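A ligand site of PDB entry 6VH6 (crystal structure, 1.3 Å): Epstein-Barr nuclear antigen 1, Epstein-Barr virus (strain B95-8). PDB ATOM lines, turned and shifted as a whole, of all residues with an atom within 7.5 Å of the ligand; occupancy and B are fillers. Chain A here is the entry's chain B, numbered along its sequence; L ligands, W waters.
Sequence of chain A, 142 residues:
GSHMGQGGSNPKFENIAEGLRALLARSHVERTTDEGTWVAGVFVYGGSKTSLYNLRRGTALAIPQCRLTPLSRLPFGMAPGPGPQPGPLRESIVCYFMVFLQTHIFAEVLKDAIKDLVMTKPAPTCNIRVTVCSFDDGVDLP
Water W3 lies within hydrogen-bond range of an oxygen (O1) of the ligand and the side-chain amino group of Lys 121.
Lys 12 touches the ligand. Ile 16 touches the ligand. Ser 51 touches the ligand. Leu 55 touches the ligand (CB to C4, 3.9 Å). Leu 117 touches the ligand. CG of Lys 121 touches C8 of the ligand, at 3.99 Å. Of the 25 residues printed, 8 come within 4 Å of the ligand.
The side-chain amide nitrogen (ND2) of Asn 54 sits at hydrogen-bond distance from an oxygen (O2) of the ligand, at 2.9 Å. The side-chain hydroxyl (OG1) of Thr 125 sits at hydrogen-bond distance from an oxygen (O3) of the ligand, 3.5 Å away.
The side-chain amide nitrogen (ND2) of Asn 54 lies close to the backbone carbonyl oxygen (O) of Thr 50 (3.3 Å). The side-chain hydroxyl (OG) of Ser 51 sits at hydrogen-bond distance from the side-chain hydroxyl (OG) of Ser 48 (2.9 Å). The side-chain hydroxyl of Thr 120 lies within hydrogen-bond range of the backbone carbonyl oxygen of Leu 117 (2.8 Å). SG of Cys 126 lies close to O of Lys 121, 3.6 Å away.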
ATOM      1  N   LYS A  12      24.301 -12.891  -0.652  1.00  0.00           N
ATOM      2  CA  LYS A  12      23.725 -11.548  -0.719  1.00  0.00           C
ATOM      3  C   LYS A  12      22.643 -11.353   0.344  1.00  0.00           C
ATOM      4  O   LYS A  12      22.673 -10.366   1.091  1.00  0.00           O
ATOM      5  CB  LYS A  12      23.190 -11.238  -2.126  1.00  0.00           C
ATOM      6  CG  LYS A  12      22.786  -9.775  -2.268  1.00  0.00           C
ATOM      7  CD  LYS A  12      22.768  -9.343  -3.739  1.00  0.00           C
ATOM      8  CE  LYS A  12      23.082  -7.854  -3.880  1.00  0.00           C
ATOM      9  NZ  LYS A  12      23.158  -7.424  -5.316  1.00  0.00           N
ATOM     10  N   ASN A  15      24.173 -11.494   3.910  1.00  0.00           N
ATOM     11  CA  ASN A  15      24.981 -10.335   4.269  1.00  0.00           C
ATOM     12  C   ASN A  15      24.089  -9.160   4.636  1.00  0.00           C
ATOM     13  O   ASN A  15      24.407  -8.411   5.569  1.00  0.00           O
ATOM     14  CB  ASN A  15      25.990 -10.019   3.154  1.00  0.00           C
ATOM     15  CG  ASN A  15      27.070 -11.099   3.034  1.00  0.00           C
ATOM     16  OD1 ASN A  15      27.319 -11.845   3.985  1.00  0.00           O
ATOM     17  ND2 ASN A  15      27.692 -11.195   1.858  1.00  0.00           N
ATOM     18  N   ILE A  16      22.943  -9.007   3.972  1.00  0.00           N
ATOM     19  CA  ILE A  16      21.971  -8.005   4.397  1.00  0.00           C
ATOM     20  C   ILE A  16      21.416  -8.364   5.766  1.00  0.00           C
ATOM     21  O   ILE A  16      21.297  -7.509   6.654  1.00  0.00           O
ATOM     22  CB  ILE A  16      20.853  -7.860   3.343  1.00  0.00           C
ATOM     23  CG1 ILE A  16      21.439  -7.307   2.035  1.00  0.00           C
ATOM     24  CG2 ILE A  16      19.731  -6.970   3.853  1.00  0.00           C
ATOM     25  CD1 ILE A  16      20.522  -7.512   0.828  1.00  0.00           C
ATOM     26  N   ALA A  17      21.077  -9.633   5.970  1.00  0.00           N
ATOM     27  CA  ALA A  17      20.584 -10.069   7.274  1.00  0.00           C
ATOM     28  C   ALA A  17      21.593  -9.749   8.364  1.00  0.00           C
ATOM     29  O   ALA A  17      21.215  -9.310   9.472  1.00  0.00           O
ATOM     30  CB  ALA A  17      20.294 -11.564   7.239  1.00  0.00           C
ATOM     31  N   GLY A  19      23.890  -7.366   8.376  1.00  0.00           N
ATOM     32  CA  GLY A  19      23.897  -5.932   8.610  1.00  0.00           C
ATOM     33  C   GLY A  19      22.746  -5.519   9.471  1.00  0.00           C
ATOM     34  O   GLY A  19      22.885  -4.690  10.394  1.00  0.00           O
ATOM     35  N   LEU A  20      21.555  -6.073   9.220  1.00  0.00           N
ATOM     36  CA  LEU A  20      20.399  -5.777  10.038  1.00  0.00           C
ATOM     37  C   LEU A  20      20.577  -6.300  11.454  1.00  0.00           C
ATOM     38  O   LEU A  20      20.328  -5.571  12.425  1.00  0.00           O
ATOM     39  CB  LEU A  20      19.152  -6.397   9.394  1.00  0.00           C
ATOM     40  CG  LEU A  20      18.249  -5.465   8.601  1.00  0.00           C
ATOM     41  CD1 LEU A  20      17.255  -6.293   7.803  1.00  0.00           C
ATOM     42  CD2 LEU A  20      17.560  -4.519   9.571  1.00  0.00           C
ATOM     43  N   SER A  48      14.633   0.412  -5.561  1.00  0.00           N
ATOM     44  CA  SER A  48      14.325  -0.225  -6.825  1.00  0.00           C
ATOM     45  C   SER A  48      13.663  -1.548  -6.476  1.00  0.00           C
ATOM     46  O   SER A  48      13.711  -2.004  -5.330  1.00  0.00           O
ATOM     47  CB  SER A  48      15.588  -0.509  -7.625  1.00  0.00           C
ATOM     48  OG  SER A  48      16.355  -1.500  -6.956  1.00  0.00           O
ATOM     49  N   THR A  50      14.494  -4.566  -7.290  1.00  0.00           N
ATOM     50  CA  THR A  50      15.464  -5.577  -6.868  1.00  0.00           C
ATOM     51  C   THR A  50      16.035  -5.276  -5.495  1.00  0.00           C
ATOM     52  O   THR A  50      16.158  -6.183  -4.658  1.00  0.00           O
ATOM     53  CB  THR A  50      16.547  -5.697  -7.926  1.00  0.00           C
ATOM     54  OG1 THR A  50      15.966  -6.118  -9.157  1.00  0.00           O
ATOM     55  CG2 THR A  50      17.593  -6.701  -7.475  1.00  0.00           C
ATOM     56  N   SER A  51      16.392  -4.021  -5.222  1.00  0.00           N
ATOM     57  CA  SER A  51      16.970  -3.699  -3.916  1.00  0.00           C
ATOM     58  C   SER A  51      15.951  -3.913  -2.810  1.00  0.00           C
ATOM     59  O   SER A  51      16.293  -4.392  -1.738  1.00  0.00           O
ATOM     60  CB  SER A  51      17.590  -2.295  -3.881  1.00  0.00           C
ATOM     61  OG  SER A  51      16.632  -1.301  -4.076  1.00  0.00           O
ATOM     62  N   LEU A  52      14.681  -3.605  -3.071  1.00  0.00           N
ATOM     63  CA  LEU A  52      13.668  -3.858  -2.057  1.00  0.00           C
ATOM     64  C   LEU A  52      13.504  -5.343  -1.830  1.00  0.00           C
ATOM     65  O   LEU A  52      13.358  -5.805  -0.695  1.00  0.00           O
ATOM     66  CB  LEU A  52      12.337  -3.262  -2.490  1.00  0.00           C
ATOM     67  CG  LEU A  52      11.970  -1.842  -2.160  1.00  0.00           C
ATOM     68  CD1 LEU A  52      10.615  -1.565  -2.838  1.00  0.00           C
ATOM     69  CD2 LEU A  52      11.900  -1.670  -0.644  1.00  0.00           C
ATOM     70  N   TYR A  53      13.449  -6.131  -2.913  1.00  0.00           N
ATOM     71  CA  TYR A  53      13.367  -7.572  -2.789  1.00  0.00           C
ATOM     72  C   TYR A  53      14.512  -8.120  -1.951  1.00  0.00           C
ATOM     73  O   TYR A  53      14.298  -8.941  -1.045  1.00  0.00           O
ATOM     74  CB  TYR A  53      13.348  -8.192  -4.194  1.00  0.00           C
ATOM     75  CG  TYR A  53      13.304  -9.678  -4.145  1.00  0.00           C
ATOM     76  CD1 TYR A  53      12.098 -10.376  -4.128  1.00  0.00           C
ATOM     77  CD2 TYR A  53      14.476 -10.408  -4.061  1.00  0.00           C
ATOM     78  CE1 TYR A  53      12.080 -11.784  -4.059  1.00  0.00           C
ATOM     79  CE2 TYR A  53      14.474 -11.758  -3.964  1.00  0.00           C
ATOM     80  CZ  TYR A  53      13.280 -12.443  -3.964  1.00  0.00           C
ATOM     81  OH  TYR A  53      13.351 -13.818  -3.889  1.00  0.00           O
ATOM     82  N   ASN A  54      15.724  -7.660  -2.217  1.00  0.00           N
ATOM     83  CA  ASN A  54      16.877  -8.138  -1.460  1.00  0.00           C
ATOM     84  C   ASN A  54      16.757  -7.763   0.011  1.00  0.00           C
ATOM     85  O   ASN A  54      17.067  -8.582   0.905  1.00  0.00           O
ATOM     86  CB  ASN A  54      18.152  -7.557  -2.067  1.00  0.00           C
ATOM     87  CG  ASN A  54      18.442  -8.136  -3.442  1.00  0.00           C
ATOM     88  OD1 ASN A  54      17.980  -9.224  -3.793  1.00  0.00           O
ATOM     89  ND2 ASN A  54      19.226  -7.394  -4.231  1.00  0.00           N
ATOM     90  N   LEU A  55      16.297  -6.546   0.298  1.00  0.00           N
ATOM     91  CA  LEU A  55      16.092  -6.158   1.694  1.00  0.00           C
ATOM     92  C   LEU A  55      15.033  -7.041   2.363  1.00  0.00           C
ATOM     93  O   LEU A  55      15.186  -7.426   3.531  1.00  0.00           O
ATOM     94  CB  LEU A  55      15.697  -4.688   1.777  1.00  0.00           C
ATOM     95  CG  LEU A  55      15.392  -4.183   3.190  1.00  0.00           C
ATOM     96  CD1 LEU A  55      16.548  -4.346   4.145  1.00  0.00           C
ATOM     97  CD2 LEU A  55      14.938  -2.710   3.127  1.00  0.00           C
ATOM     98  N   ARG A  56      13.962  -7.344   1.654  1.00  0.00           N
ATOM     99  CA  ARG A  56      12.912  -8.217   2.170  1.00  0.00           C
ATOM    100  C   ARG A  56      13.468  -9.583   2.520  1.00  0.00           C
ATOM    101  O   ARG A  56      13.159 -10.133   3.590  1.00  0.00           O
ATOM    102  CB  ARG A  56      11.788  -8.313   1.128  1.00  0.00           C
ATOM    103  CG  ARG A  56      10.673  -9.274   1.364  1.00  0.00           C
ATOM    104  CD  ARG A  56       9.586  -9.096   0.274  1.00  0.00           C
ATOM    105  NE  ARG A  56       8.617 -10.196   0.306  1.00  0.00           N
ATOM    106  CZ  ARG A  56       8.811 -11.377  -0.241  1.00  0.00           C
ATOM    107  NH1 ARG A  56       9.940 -11.600  -0.908  1.00  0.00           N
ATOM    108  NH2 ARG A  56       7.870 -12.318  -0.153  1.00  0.00           N
ATOM    109  N   ILE A 114      16.534  -0.158   9.605  1.00  0.00           N
ATOM    110  CA  ILE A 114      16.516  -0.104   8.151  1.00  0.00           C
ATOM    111  C   ILE A 114      17.080   1.207   7.658  1.00  0.00           C
ATOM    112  O   ILE A 114      17.886   1.230   6.728  1.00  0.00           O
ATOM    113  CB  ILE A 114      15.095  -0.372   7.628  1.00  0.00           C
ATOM    114  CG1 ILE A 114      14.737  -1.825   7.904  1.00  0.00           C
ATOM    115  CG2 ILE A 114      14.986  -0.012   6.137  1.00  0.00           C
ATOM    116  CD1 ILE A 114      13.244  -2.146   7.661  1.00  0.00           C
ATOM    117  N   LEU A 117      20.794   1.126   8.018  1.00  0.00           N
ATOM    118  CA  LEU A 117      21.466   0.180   7.137  1.00  0.00           C
ATOM    119  C   LEU A 117      21.530   0.705   5.708  1.00  0.00           C
ATOM    120  O   LEU A 117      22.593   0.680   5.075  1.00  0.00           O
ATOM    121  CB  LEU A 117      20.715  -1.145   7.191  1.00  0.00           C
ATOM    122  CG  LEU A 117      21.440  -2.217   6.384  1.00  0.00           C
ATOM    123  CD1 LEU A 117      22.851  -2.484   6.847  1.00  0.00           C
ATOM    124  CD2 LEU A 117      20.624  -3.510   6.413  1.00  0.00           C
ATOM    125  N   VAL A 118      20.408   1.193   5.177  1.00  0.00           N
ATOM    126  CA  VAL A 118      20.393   1.546   3.759  1.00  0.00           C
ATOM    127  C   VAL A 118      21.224   2.801   3.468  1.00  0.00           C
ATOM    128  O   VAL A 118      21.712   2.959   2.345  1.00  0.00           O
ATOM    129  CB  VAL A 118      18.989   1.651   3.167  1.00  0.00           C
ATOM    130  CG1 VAL A 118      18.229   0.331   3.309  1.00  0.00           C
ATOM    131  CG2 VAL A 118      18.193   2.777   3.766  1.00  0.00           C
ATOM    132  N   MET A 119      21.414   3.686   4.460  1.00  0.00           N
ATOM    133  CA  MET A 119      22.142   4.914   4.170  1.00  0.00           C
ATOM    134  C   MET A 119      23.615   4.665   3.925  1.00  0.00           C
ATOM    135  O   MET A 119      24.283   5.561   3.415  1.00  0.00           O
ATOM    136  CB  MET A 119      21.926   5.962   5.261  1.00  0.00           C
ATOM    137  CG  MET A 119      22.491   5.646   6.618  1.00  0.00           C
ATOM    138  SD  MET A 119      22.518   7.138   7.667  1.00  0.00           S
ATOM    139  CE  MET A 119      20.738   7.342   7.940  1.00  0.00           C
ATOM    140  N   THR A 120      24.129   3.481   4.254  1.00  0.00           N
ATOM    141  CA  THR A 120      25.520   3.139   4.013  1.00  0.00           C
ATOM    142  C   THR A 120      25.744   2.494   2.641  1.00  0.00           C
ATOM    143  O   THR A 120      26.881   2.105   2.336  1.00  0.00           O
ATOM    144  CB  THR A 120      26.039   2.181   5.099  1.00  0.00           C
ATOM    145  OG1 THR A 120      25.422   0.908   4.927  1.00  0.00           O
ATOM    146  CG2 THR A 120      25.741   2.723   6.493  1.00  0.00           C
ATOM    147  N   LYS A 121      24.703   2.400   1.814  1.00  0.00           N
ATOM    148  CA  LYS A 121      24.799   1.691   0.551  1.00  0.00           C
ATOM    149  C   LYS A 121      24.642   2.671  -0.602  1.00  0.00           C
ATOM    150  O   LYS A 121      24.009   3.717  -0.452  1.00  0.00           O
ATOM    151  CB  LYS A 121      23.672   0.657   0.459  1.00  0.00           C
ATOM    152  CG  LYS A 121      23.610  -0.298   1.638  1.00  0.00           C
ATOM    153  CD  LYS A 121      24.948  -0.961   1.845  1.00  0.00           C
ATOM    154  CE  LYS A 121      24.873  -1.941   3.001  1.00  0.00           C
ATOM    155  NZ  LYS A 121      26.184  -2.610   3.230  1.00  0.00           N
ATOM    156  N   PRO A 122      25.161   2.344  -1.784  1.00  0.00           N
ATOM    157  CA  PRO A 122      24.959   3.224  -2.947  1.00  0.00           C
ATOM    158  C   PRO A 122      23.536   3.144  -3.467  1.00  0.00           C
ATOM    159  O   PRO A 122      22.766   2.222  -3.161  1.00  0.00           O
ATOM    160  CB  PRO A 122      25.964   2.701  -3.973  1.00  0.00           C
ATOM    161  CG  PRO A 122      26.227   1.310  -3.580  1.00  0.00           C
ATOM    162  CD  PRO A 122      26.024   1.194  -2.099  1.00  0.00           C
ATOM    163  N   PRO A 124      20.599   2.314  -5.941  1.00  0.00           N
ATOM    164  CA  PRO A 124      19.353   2.861  -5.426  1.00  0.00           C
ATOM    165  C   PRO A 124      18.977   2.434  -4.009  1.00  0.00           C
ATOM    166  O   PRO A 124      17.951   2.871  -3.498  1.00  0.00           O
ATOM    167  CB  PRO A 124      18.310   2.303  -6.395  1.00  0.00           C
ATOM    168  CG  PRO A 124      18.877   0.974  -6.815  1.00  0.00           C
ATOM    169  CD  PRO A 124      20.397   1.178  -6.860  1.00  0.00           C
ATOM    170  N   THR A 125      19.788   1.585  -3.375  1.00  0.00           N
ATOM    171  CA  THR A 125      19.437   1.066  -2.066  1.00  0.00           C
ATOM    172  C   THR A 125      19.248   2.177  -1.049  1.00  0.00           C
ATOM    173  O   THR A 125      18.334   2.118  -0.216  1.00  0.00           O
ATOM    174  CB  THR A 125      20.503   0.071  -1.606  1.00  0.00           C
ATOM    175  OG1 THR A 125      20.508  -1.023  -2.519  1.00  0.00           O
ATOM    176  CG2 THR A 125      20.207  -0.411  -0.218  1.00  0.00           C
ATOM    177  N   CYS A 126      20.108   3.203  -1.079  1.00  0.00           N
ATOM    178  CA  CYS A 126      19.980   4.294  -0.124  1.00  0.00           C
ATOM    179  C   CYS A 126      18.701   5.099  -0.295  1.00  0.00           C
ATOM    180  O   CYS A 126      18.388   5.925   0.571  1.00  0.00           O
ATOM    181  CB  CYS A 126      21.227   5.188  -0.136  1.00  0.00           C
ATOM    182  SG  CYS A 126      21.537   5.932  -1.717  1.00  0.00           S
ATOM    183  N   ILE A 128      15.708   3.714  -0.470  1.00  0.00           N
ATOM    184  CA  ILE A 128      14.626   3.014   0.202  1.00  0.00           C
ATOM    185  C   ILE A 128      14.177   3.852   1.374  1.00  0.00           C
ATOM    186  O   ILE A 128      14.990   4.439   2.115  1.00  0.00           O
ATOM    187  CB  ILE A 128      15.097   1.623   0.645  1.00  0.00           C
ATOM    188  CG1 ILE A 128      15.350   0.745  -0.589  1.00  0.00           C
ATOM    189  CG2 ILE A 128      14.117   0.998   1.620  1.00  0.00           C
ATOM    190  CD1 ILE A 128      15.983  -0.608  -0.293  1.00  0.00           C
HETATM  191  C1  LIG L   1      22.305  -4.547  -2.836  1.00  0.00           C
HETATM  192  C2  LIG L   1      20.992  -3.201   3.122  1.00  0.00           C
HETATM  193  C3  LIG L   1      20.750  -3.545   1.667  1.00  0.00           C
HETATM  194  C4  LIG L   1      19.422  -3.648   1.171  1.00  0.00           C
HETATM  195  C5  LIG L   1      19.186  -3.944  -0.172  1.00  0.00           C
HETATM  196  C6  LIG L   1      20.273  -4.158  -0.998  1.00  0.00           C
HETATM  197  C7  LIG L   1      21.583  -4.068  -0.566  1.00  0.00           C
HETATM  198  C8  LIG L   1      21.820  -3.754   0.779  1.00  0.00           C
HETATM  199  C9  LIG L   1      22.640  -4.308  -1.553  1.00  0.00           C
HETATM  200  C10 LIG L   1      20.905  -4.617  -3.279  1.00  0.00           C
HETATM  201  O1  LIG L   1      23.923  -4.100  -1.107  1.00  0.00           O
HETATM  202  O2  LIG L   1      20.557  -4.779  -4.446  1.00  0.00           O
HETATM  203  O3  LIG L   1      19.954  -4.452  -2.319  1.00  0.00           O
HETATM  204  O   HOH W   1      25.052  -6.544  -1.877  1.00  0.00           O
HETATM  205  O   HOH W   2      20.521  -3.067  -6.527  1.00  0.00           O
HETATM  206  O   HOH W   3      25.800  -4.384   0.838  1.00  0.00           O
HETATM  207  O   HOH W   4      25.197  -2.173  -2.605  1.00  0.00           O
